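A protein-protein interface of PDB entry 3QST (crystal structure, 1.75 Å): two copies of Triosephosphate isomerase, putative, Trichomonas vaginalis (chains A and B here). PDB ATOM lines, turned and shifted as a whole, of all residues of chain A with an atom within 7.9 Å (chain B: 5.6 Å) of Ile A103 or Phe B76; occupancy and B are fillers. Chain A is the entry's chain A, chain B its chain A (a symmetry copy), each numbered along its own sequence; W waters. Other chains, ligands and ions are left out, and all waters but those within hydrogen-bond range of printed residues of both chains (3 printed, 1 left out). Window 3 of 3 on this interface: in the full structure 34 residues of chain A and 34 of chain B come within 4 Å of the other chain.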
ATOM      1  N   ASN A  12      23.322 -12.918 -15.867  1.00  0.00           N
ATOM      2  CA  ASN A  12      23.456 -14.260 -15.307  1.00  0.00           C
ATOM      3  C   ASN A  12      24.798 -14.404 -14.613  1.00  0.00           C
ATOM      4  O   ASN A  12      25.819 -14.625 -15.267  1.00  0.00           O
ATOM      5  CB  ASN A  12      23.329 -15.302 -16.433  1.00  0.00           C
ATOM      6  CG  ASN A  12      23.395 -16.726 -15.923  1.00  0.00           C
ATOM      7  OD1 ASN A  12      23.334 -16.972 -14.711  1.00  0.00           O
ATOM      8  ND2 ASN A  12      23.503 -17.683 -16.851  1.00  0.00           N
ATOM      9  N   TRP A  13      24.816 -14.283 -13.289  1.00  0.00           N
ATOM     10  CA  TRP A  13      26.064 -14.453 -12.554  1.00  0.00           C
ATOM     11  C   TRP A  13      26.623 -15.871 -12.651  1.00  0.00           C
ATOM     12  O   TRP A  13      27.795 -16.089 -12.331  1.00  0.00           O
ATOM     13  CB  TRP A  13      25.872 -14.147 -11.081  1.00  0.00           C
ATOM     14  CG  TRP A  13      25.581 -12.734 -10.782  1.00  0.00           C
ATOM     15  CD1 TRP A  13      25.312 -11.723 -11.674  1.00  0.00           C
ATOM     16  CD2 TRP A  13      25.538 -12.150  -9.484  1.00  0.00           C
ATOM     17  NE1 TRP A  13      25.106 -10.540 -10.988  1.00  0.00           N
ATOM     18  CE2 TRP A  13      25.236 -10.784  -9.645  1.00  0.00           C
ATOM     19  CE3 TRP A  13      25.721 -12.661  -8.189  1.00  0.00           C
ATOM     20  CZ2 TRP A  13      25.118  -9.916  -8.557  1.00  0.00           C
ATOM     21  CZ3 TRP A  13      25.605 -11.799  -7.119  1.00  0.00           C
ATOM     22  CH2 TRP A  13      25.309 -10.442  -7.311  1.00  0.00           C
ATOM     23  N   LYS A  14      25.791 -16.820 -13.073  1.00  0.00           N
ATOM     24  CA  LYS A  14      26.172 -18.245 -13.084  1.00  0.00           C
ATOM     25  C   LYS A  14      26.611 -18.672 -11.677  1.00  0.00           C
ATOM     26  O   LYS A  14      26.005 -18.227 -10.698  1.00  0.00           O
ATOM     27  CB  LYS A  14      27.227 -18.539 -14.152  1.00  0.00           C
ATOM     28  CG  LYS A  14      26.805 -18.051 -15.550  1.00  0.00           C
ATOM     29  CD  LYS A  14      27.814 -18.483 -16.614  1.00  0.00           C
ATOM     30  CE  LYS A  14      27.351 -18.064 -18.023  1.00  0.00           C
ATOM     31  NZ  LYS A  14      28.227 -18.648 -19.103  1.00  0.00           N
ATOM     32  N   ALA A  15      27.614 -19.544 -11.556  1.00  0.00           N
ATOM     33  CA  ALA A  15      28.036 -19.975 -10.217  1.00  0.00           C
ATOM     34  C   ALA A  15      29.118 -19.038  -9.684  1.00  0.00           C
ATOM     35  O   ALA A  15      30.267 -19.438  -9.502  1.00  0.00           O
ATOM     36  CB  ALA A  15      28.529 -21.440 -10.220  1.00  0.00           C
ATOM     37  N   ASN A  16      28.735 -17.779  -9.464  1.00  0.00           N
ATOM     38  CA  ASN A  16      29.642 -16.728  -9.020  1.00  0.00           C
ATOM     39  C   ASN A  16      28.819 -15.709  -8.231  1.00  0.00           C
ATOM     40  O   ASN A  16      27.601 -15.661  -8.382  1.00  0.00           O
ATOM     41  CB  ASN A  16      30.246 -15.999 -10.221  1.00  0.00           C
ATOM     42  CG  ASN A  16      31.081 -16.906 -11.130  1.00  0.00           C
ATOM     43  OD1 ASN A  16      32.248 -17.188 -10.853  1.00  0.00           O
ATOM     44  ND2 ASN A  16      30.499 -17.310 -12.249  1.00  0.00           N
ATOM     45  N   PRO A  46      23.318 -17.310  -7.695  1.00  0.00           N
ATOM     46  CA  PRO A  46      23.233 -18.608  -7.016  1.00  0.00           C
ATOM     47  C   PRO A  46      22.188 -18.630  -5.903  1.00  0.00           C
ATOM     48  O   PRO A  46      21.985 -17.609  -5.248  1.00  0.00           O
ATOM     49  CB  PRO A  46      24.632 -18.780  -6.423  1.00  0.00           C
ATOM     50  CG  PRO A  46      25.529 -18.016  -7.355  1.00  0.00           C
ATOM     51  CD  PRO A  46      24.702 -16.799  -7.732  1.00  0.00           C
ATOM     52  N   GLU A  66      18.475 -19.150 -11.007  1.00  0.00           N
ATOM     53  CA  GLU A  66      19.173 -19.675 -12.187  1.00  0.00           C
ATOM     54  C   GLU A  66      18.617 -21.019 -12.663  1.00  0.00           C
ATOM     55  O   GLU A  66      19.056 -21.550 -13.682  1.00  0.00           O
ATOM     56  CB  GLU A  66      20.672 -19.818 -11.909  1.00  0.00           C
ATOM     57  CG  GLU A  66      21.375 -18.450 -11.805  1.00  0.00           C
ATOM     58  CD  GLU A  66      22.854 -18.566 -11.518  1.00  0.00           C
ATOM     59  OE1 GLU A  66      23.414 -19.661 -11.773  1.00  0.00           O
ATOM     60  OE2 GLU A  66      23.460 -17.561 -11.028  1.00  0.00           O
ATOM     61  N   HIS A  97      19.261 -23.250 -19.526  1.00  0.00           N
ATOM     62  CA  HIS A  97      20.590 -22.746 -19.880  1.00  0.00           C
ATOM     63  C   HIS A  97      21.451 -23.880 -20.434  1.00  0.00           C
ATOM     64  O   HIS A  97      21.360 -25.014 -19.954  1.00  0.00           O
ATOM     65  CB  HIS A  97      21.290 -22.110 -18.679  1.00  0.00           C
ATOM     66  CG  HIS A  97      22.470 -21.273 -19.061  1.00  0.00           C
ATOM     67  ND1 HIS A  97      23.719 -21.803 -19.304  1.00  0.00           N
ATOM     68  CD2 HIS A  97      22.577 -19.940 -19.279  1.00  0.00           C
ATOM     69  CE1 HIS A  97      24.548 -20.832 -19.649  1.00  0.00           C
ATOM     70  NE2 HIS A  97      23.882 -19.690 -19.633  1.00  0.00           N
ATOM     71  N   SER A  98      22.250 -23.571 -21.459  1.00  0.00           N
ATOM     72  CA  SER A  98      23.123 -24.547 -22.106  1.00  0.00           C
ATOM     73  C   SER A  98      23.956 -25.337 -21.105  1.00  0.00           C
ATOM     74  O   SER A  98      24.198 -26.531 -21.290  1.00  0.00           O
ATOM     75  CB  SER A  98      24.058 -23.860 -23.122  1.00  0.00           C
ATOM     76  OG  SER A  98      24.916 -22.922 -22.485  1.00  0.00           O
ATOM     77  N   GLU A  99      24.403 -24.671 -20.045  1.00  0.00           N
ATOM     78  CA  GLU A  99      25.244 -25.347 -19.057  1.00  0.00           C
ATOM     79  C   GLU A  99      24.452 -26.435 -18.333  1.00  0.00           C
ATOM     80  O   GLU A  99      24.995 -27.483 -17.992  1.00  0.00           O
ATOM     81  CB  GLU A  99      25.852 -24.319 -18.073  1.00  0.00           C
ATOM     82  CG  GLU A  99      26.926 -23.483 -18.756  1.00  0.00           C
ATOM     83  CD  GLU A  99      27.095 -22.103 -18.161  1.00  0.00           C
ATOM     84  OE1 GLU A  99      26.534 -21.826 -17.075  1.00  0.00           O
ATOM     85  OE2 GLU A  99      27.778 -21.290 -18.804  1.00  0.00           O
ATOM     86  N   ARG A 100      23.162 -26.194 -18.097  1.00  0.00           N
ATOM     87  CA  ARG A 100      22.344 -27.204 -17.433  1.00  0.00           C
ATOM     88  C   ARG A 100      21.941 -28.303 -18.406  1.00  0.00           C
ATOM     89  O   ARG A 100      21.867 -29.465 -18.034  1.00  0.00           O
ATOM     90  CB  ARG A 100      21.107 -26.574 -16.783  1.00  0.00           C
ATOM     91  CG  ARG A 100      21.498 -25.570 -15.696  1.00  0.00           C
ATOM     92  CD  ARG A 100      20.451 -25.478 -14.570  1.00  0.00           C
ATOM     93  NE  ARG A 100      20.302 -26.742 -13.842  1.00  0.00           N
ATOM     94  CZ  ARG A 100      21.131 -27.179 -12.897  1.00  0.00           C
ATOM     95  NH1 ARG A 100      22.192 -26.457 -12.546  1.00  0.00           N
ATOM     96  NH2 ARG A 100      20.888 -28.347 -12.295  1.00  0.00           N
ATOM     97  N   ARG A 101      21.673 -27.936 -19.654  1.00  0.00           N
ATOM     98  CA  ARG A 101      21.306 -28.946 -20.642  1.00  0.00           C
ATOM     99  C   ARG A 101      22.478 -29.875 -20.890  1.00  0.00           C
ATOM    100  O   ARG A 101      22.312 -31.079 -21.098  1.00  0.00           O
ATOM    101  CB  ARG A 101      20.936 -28.284 -21.959  1.00  0.00           C
ATOM    102  CG  ARG A 101      19.600 -27.572 -21.947  1.00  0.00           C
ATOM    103  CD  ARG A 101      19.377 -26.969 -23.321  1.00  0.00           C
ATOM    104  NE  ARG A 101      18.159 -26.181 -23.470  1.00  0.00           N
ATOM    105  CZ  ARG A 101      17.040 -26.611 -24.046  1.00  0.00           C
ATOM    106  NH1 ARG A 101      16.937 -27.876 -24.470  1.00  0.00           N
ATOM    107  NH2 ARG A 101      16.011 -25.783 -24.181  1.00  0.00           N
ATOM    108  N   ASP A 102      23.669 -29.303 -20.897  1.00  0.00           N
ATOM    109  CA  ASP A 102      24.836 -30.075 -21.300  1.00  0.00           C
ATOM    110  C   ASP A 102      25.558 -30.730 -20.103  1.00  0.00           C
ATOM    111  O   ASP A 102      25.681 -31.957 -20.045  1.00  0.00           O
ATOM    112  CB  ASP A 102      25.734 -29.230 -22.227  1.00  0.00           C
ATOM    113  CG  ASP A 102      24.986 -28.762 -23.504  1.00  0.00           C
ATOM    114  OD1 ASP A 102      24.051 -29.471 -23.957  1.00  0.00           O
ATOM    115  OD2 ASP A 102      25.317 -27.685 -24.056  1.00  0.00           O
ATOM    116  N   ILE A 103      25.988 -29.939 -19.126  1.00  0.00           N
ATOM    117  CA  ILE A 103      26.685 -30.499 -17.968  1.00  0.00           C
ATOM    118  C   ILE A 103      25.769 -31.284 -17.019  1.00  0.00           C
ATOM    119  O   ILE A 103      26.122 -32.381 -16.588  1.00  0.00           O
ATOM    120  CB  ILE A 103      27.466 -29.413 -17.183  1.00  0.00           C
ATOM    121  CG1 ILE A 103      28.473 -28.712 -18.097  1.00  0.00           C
ATOM    122  CG2 ILE A 103      28.183 -30.029 -15.996  1.00  0.00           C
ATOM    123  CD1 ILE A 103      29.003 -27.399 -17.524  1.00  0.00           C
ATOM    124  N   LEU A 104      24.594 -30.735 -16.701  1.00  0.00           N
ATOM    125  CA  LEU A 104      23.678 -31.398 -15.776  1.00  0.00           C
ATOM    126  C   LEU A 104      22.635 -32.261 -16.499  1.00  0.00           C
ATOM    127  O   LEU A 104      21.728 -32.807 -15.873  1.00  0.00           O
ATOM    128  CB  LEU A 104      23.008 -30.389 -14.812  1.00  0.00           C
ATOM    129  CG  LEU A 104      23.887 -29.767 -13.708  1.00  0.00           C
ATOM    130  CD1 LEU A 104      24.831 -30.819 -13.104  1.00  0.00           C
ATOM    131  CD2 LEU A 104      24.717 -28.586 -14.194  1.00  0.00           C
ATOM    132  N   LYS A 105      22.780 -32.381 -17.815  1.00  0.00           N
ATOM    133  CA  LYS A 105      21.970 -33.310 -18.608  1.00  0.00           C
ATOM    134  C   LYS A 105      20.459 -33.076 -18.555  1.00  0.00           C
ATOM    135  O   LYS A 105      19.678 -34.031 -18.566  1.00  0.00           O
ATOM    136  CB  LYS A 105      22.281 -34.768 -18.221  1.00  0.00           C
ATOM    137  N   GLU A 106      20.038 -31.816 -18.518  1.00  0.00           N
ATOM    138  CA  GLU A 106      18.616 -31.513 -18.528  1.00  0.00           C
ATOM    139  C   GLU A 106      18.067 -31.632 -19.952  1.00  0.00           C
ATOM    140  O   GLU A 106      18.540 -30.950 -20.859  1.00  0.00           O
ATOM    141  CB  GLU A 106      18.374 -30.113 -17.935  1.00  0.00           C
ATOM    142  CG  GLU A 106      18.802 -30.023 -16.475  1.00  0.00           C
ATOM    143  CD  GLU A 106      18.229 -28.814 -15.743  1.00  0.00           C
ATOM    144  OE1 GLU A 106      17.530 -28.008 -16.376  1.00  0.00           O
ATOM    145  OE2 GLU A 106      18.493 -28.684 -14.530  1.00  0.00           O
ATOM    146  N   PHE B  69      28.400 -28.499  -5.886  1.00  0.00           N
ATOM    147  CA  PHE B  69      29.033 -28.837  -7.160  1.00  0.00           C
ATOM    148  C   PHE B  69      30.503 -29.236  -6.942  1.00  0.00           C
ATOM    149  O   PHE B  69      30.987 -29.314  -5.806  1.00  0.00           O
ATOM    150  CB  PHE B  69      28.863 -27.659  -8.154  1.00  0.00           C
ATOM    151  CG  PHE B  69      29.212 -27.992  -9.588  1.00  0.00           C
ATOM    152  CD1 PHE B  69      28.559 -29.024 -10.275  1.00  0.00           C
ATOM    153  CD2 PHE B  69      30.171 -27.241 -10.260  1.00  0.00           C
ATOM    154  CE1 PHE B  69      28.886 -29.314 -11.598  1.00  0.00           C
ATOM    155  CE2 PHE B  69      30.516 -27.531 -11.574  1.00  0.00           C
ATOM    156  CZ  PHE B  69      29.870 -28.566 -12.250  1.00  0.00           C
ATOM    157  N   LYS B  71      33.290 -27.655  -8.310  1.00  0.00           N
ATOM    158  CA  LYS B  71      34.258 -26.596  -8.593  1.00  0.00           C
ATOM    159  C   LYS B  71      34.036 -25.414  -7.671  1.00  0.00           C
ATOM    160  O   LYS B  71      32.987 -25.311  -7.031  1.00  0.00           O
ATOM    161  CB  LYS B  71      34.140 -26.135 -10.055  1.00  0.00           C
ATOM    162  CG  LYS B  71      34.245 -27.263 -11.078  1.00  0.00           C
ATOM    163  CD  LYS B  71      35.681 -27.730 -11.255  1.00  0.00           C
ATOM    164  CE  LYS B  71      35.790 -28.732 -12.404  1.00  0.00           C
ATOM    165  NZ  LYS B  71      37.170 -29.277 -12.570  1.00  0.00           N
ATOM    166  N   ASN B  73      33.644 -22.229  -8.409  1.00  0.00           N
ATOM    167  CA  ASN B  73      32.804 -21.214  -9.021  1.00  0.00           C
ATOM    168  C   ASN B  73      32.969 -21.371 -10.515  1.00  0.00           C
ATOM    169  O   ASN B  73      33.855 -22.100 -10.970  1.00  0.00           O
ATOM    170  CB  ASN B  73      33.234 -19.798  -8.599  1.00  0.00           C
ATOM    171  CG  ASN B  73      34.628 -19.420  -9.110  1.00  0.00           C
ATOM    172  OD1 ASN B  73      35.624 -20.020  -8.717  1.00  0.00           O
ATOM    173  ND2 ASN B  73      34.698 -18.396  -9.960  1.00  0.00           N
ATOM    174  N   GLY B  74      32.130 -20.694 -11.288  1.00  0.00           N
ATOM    175  CA  GLY B  74      32.353 -20.662 -12.722  1.00  0.00           C
ATOM    176  C   GLY B  74      31.093 -20.812 -13.548  1.00  0.00           C
ATOM    177  O   GLY B  74      29.994 -20.490 -13.104  1.00  0.00           O
ATOM    178  N   ALA B  75      31.268 -21.303 -14.770  1.00  0.00           N
ATOM    179  CA  ALA B  75      30.197 -21.319 -15.756  1.00  0.00           C
ATOM    180  C   ALA B  75      29.293 -22.531 -15.573  1.00  0.00           C
ATOM    181  O   ALA B  75      29.241 -23.409 -16.431  1.00  0.00           O
ATOM    182  CB  ALA B  75      30.793 -21.291 -17.178  1.00  0.00           C
ATOM    183  N   PHE B  76      28.586 -22.562 -14.442  1.00  0.00           N
ATOM    184  CA  PHE B  76      27.771 -23.713 -14.045  1.00  0.00           C
ATOM    185  C   PHE B  76      26.434 -23.199 -13.553  1.00  0.00           C
ATOM    186  O   PHE B  76      26.110 -23.263 -12.362  1.00  0.00           O
ATOM    187  CB  PHE B  76      28.498 -24.509 -12.950  1.00  0.00           C
ATOM    188  CG  PHE B  76      29.928 -24.809 -13.300  1.00  0.00           C
ATOM    189  CD1 PHE B  76      30.229 -25.656 -14.357  1.00  0.00           C
ATOM    190  CD2 PHE B  76      30.967 -24.205 -12.612  1.00  0.00           C
ATOM    191  CE1 PHE B  76      31.551 -25.913 -14.710  1.00  0.00           C
ATOM    192  CE2 PHE B  76      32.292 -24.461 -12.964  1.00  0.00           C
ATOM    193  CZ  PHE B  76      32.578 -25.314 -13.999  1.00  0.00           C
ATOM    194  N   THR B  77      25.666 -22.641 -14.486  1.00  0.00           N
ATOM    195  CA  THR B  77      24.390 -22.018 -14.164  1.00  0.00           C
ATOM    196  C   THR B  77      23.504 -22.965 -13.362  1.00  0.00           C
ATOM    197  O   THR B  77      23.334 -24.134 -13.729  1.00  0.00           O
ATOM    198  CB  THR B  77      23.682 -21.577 -15.463  1.00  0.00           C
ATOM    199  OG1 THR B  77      24.458 -20.539 -16.061  1.00  0.00           O
ATOM    200  CG2 THR B  77      22.258 -21.062 -15.179  1.00  0.00           C
ATOM    201  N   GLY B  78      22.962 -22.461 -12.253  1.00  0.00           N
ATOM    202  CA  GLY B  78      22.101 -23.239 -11.378  1.00  0.00           C
ATOM    203  C   GLY B  78      22.810 -23.909 -10.205  1.00  0.00           C
ATOM    204  O   GLY B  78      22.147 -24.300  -9.245  1.00  0.00           O
ATOM    205  N   GLU B  79      24.134 -24.049 -10.279  1.00  0.00           N
ATOM    206  CA  GLU B  79      24.885 -24.783  -9.252  1.00  0.00           C
ATOM    207  C   GLU B  79      25.343 -23.919  -8.080  1.00  0.00           C
ATOM    208  O   GLU B  79      25.699 -22.756  -8.255  1.00  0.00           O
ATOM    209  CB  GLU B  79      26.110 -25.477  -9.858  1.00  0.00           C
ATOM    210  CG  GLU B  79      25.752 -26.603 -10.826  1.00  0.00           C
ATOM    211  CD  GLU B  79      24.896 -27.674 -10.177  1.00  0.00           C
ATOM    212  OE1 GLU B  79      25.351 -28.265  -9.174  1.00  0.00           O
ATOM    213  OE2 GLU B  79      23.765 -27.919 -10.656  1.00  0.00           O
HETATM  214  O   HOH W   1      31.734 -18.230 -14.901  1.00  0.00           O
HETATM  215  O   HOH W   2      20.901 -28.710  -8.882  1.00  0.00           O
HETATM  216  O   HOH W   3      22.314 -30.033 -10.341  1.00  0.00           O
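The side-chain carboxylate of Glu A99 sits at hydrogen-bond distance from the side-chain hydroxyl of Thr B77, 2.6 Å away. The side-chain carboxylate (OE1) of Glu A99 is in hydrogen-bond range of the backbone NH (N) of Phe B76 (3.4 Å). The side-chain amide nitrogen (ND2) of Asn A12 sits at hydrogen-bond distance from the side-chain hydroxyl (OG1) of Thr B77, at 3.1 Å. ND2 of Asn A16 lies within hydrogen-bond range of O of Gly B74 (3.3 Å). OE1 of Glu A99 lies close to O of Ala B75 (3.2 Å). The side-chain amide oxygen (OD1) of Asn A16 sits at hydrogen-bond distance from the side-chain amide nitrogen (ND2) of Asn B73 (2.9 Å). OE2 of Glu B79 is in salt-bridge range of NH1 of Arg A100, 2.9 Å away. The backbone carbonyl oxygen (O) of Thr B77 sits at hydrogen-bond distance from the guanidinium group (NH1) of Arg A100, at 2.8 Å. The backbone NH (N) of Gly B74 sits at hydrogen-bond distance from the backbone carbonyl oxygen (O) of Ala A15 (2.9 Å). The backbone NH (N) of Gly B78 sits at hydrogen-bond distance from the side-chain carboxylate (OE1) of Glu A66, 2.9 Å away.
NE2 of His A97 lies close to ND2 of Asn A12. A ring nitrogen (ND1) of His A97 lies within hydrogen-bond range of the backbone NH (N) of Glu A99, at 3.0 Å. NZ of Lys A14 is in salt-bridge range of OE2 of Glu A99 (2.7 Å). N of Lys A14 lies within hydrogen-bond range of OD1 of Asn A12. O of Arg A100 sits at hydrogen-bond distance from N of Lys A105 (3.1 Å). The guanidinium group (NE) of Arg A100 is in salt-bridge range of the side-chain carboxylate (OE2) of Glu A106, at 2.7 Å.
Among the printed residues, merely in contact across the chains: Ala A15 with Asn B73, Arg A100 with Gly B78, Lys A14 with Thr B77, Glu A66 with Thr B77, Lys A14 with Gly B74, His A97 with Thr B77, Leu A104 with Glu B79, Ala A15 with Glu B79, Ala A15 with Phe B76, Lys A14 with Ala B75 and Ile A103 with Phe B76.
Of chain B, only Phe B76 (3.8 Å) comes within 4 Å of Ile A103. Of chain A, only Ala A15, Glu A99 and Ile A103 come within 4 Å of Phe B76. Of the printed residues of chain A, Thr B77 touches Asn A12 (3.1 Å), Lys A14 (3.5 Å), Glu A66 (3.5 Å), His A97 (3.6 Å), Glu A99 (2.6 Å) and Arg A100 (2.8 Å). Printed residues of chain B within 4 Å of Asn A12: Thr B77 (3.1 Å). Of the printed residues of chain B, Ala A15 touches Asn B73, Gly B74, Phe B76 and Glu B79. The nearest printed residue of chain B that does not touch Glu A66 is Phe B76 (4.5 Å).
Of the 9 printed residues of chain B, 7 touch a printed residue of chain A. Of the 17 printed residues of chain A, 10 touch a printed residue of chain B. Hydrophobic or aromatic side chains of chain A that line the printed part of chain B: Ala A15, His A97, Ile A103 and Leu A104. Among the printed residues, 21 pairs touch across the chains. Among the printed residues, Asp or Glu carboxylates within 4 Å of a Lys or Arg side-chain nitrogen of the other chain: Arg A100 with Glu B79.
No position is printed for both chains. Of the 21 pairs that touch across the chains among the printed residues, none has its exchanged pair printed and touching as well.
Water W3 bridges OE2 of Glu B79 (2.6 Å) and NH2 of Arg A100 (2.9 Å). Water W1 lies within hydrogen-bond range of the side-chain amide nitrogen (ND2) of Asn A16, the backbone NH (N) of Ala B75 and the backbone carbonyl oxygen (O) of Gly B74. Water W2 bridges the guanidinium group of Arg A100 and the side-chain carboxylate of Glu B79.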
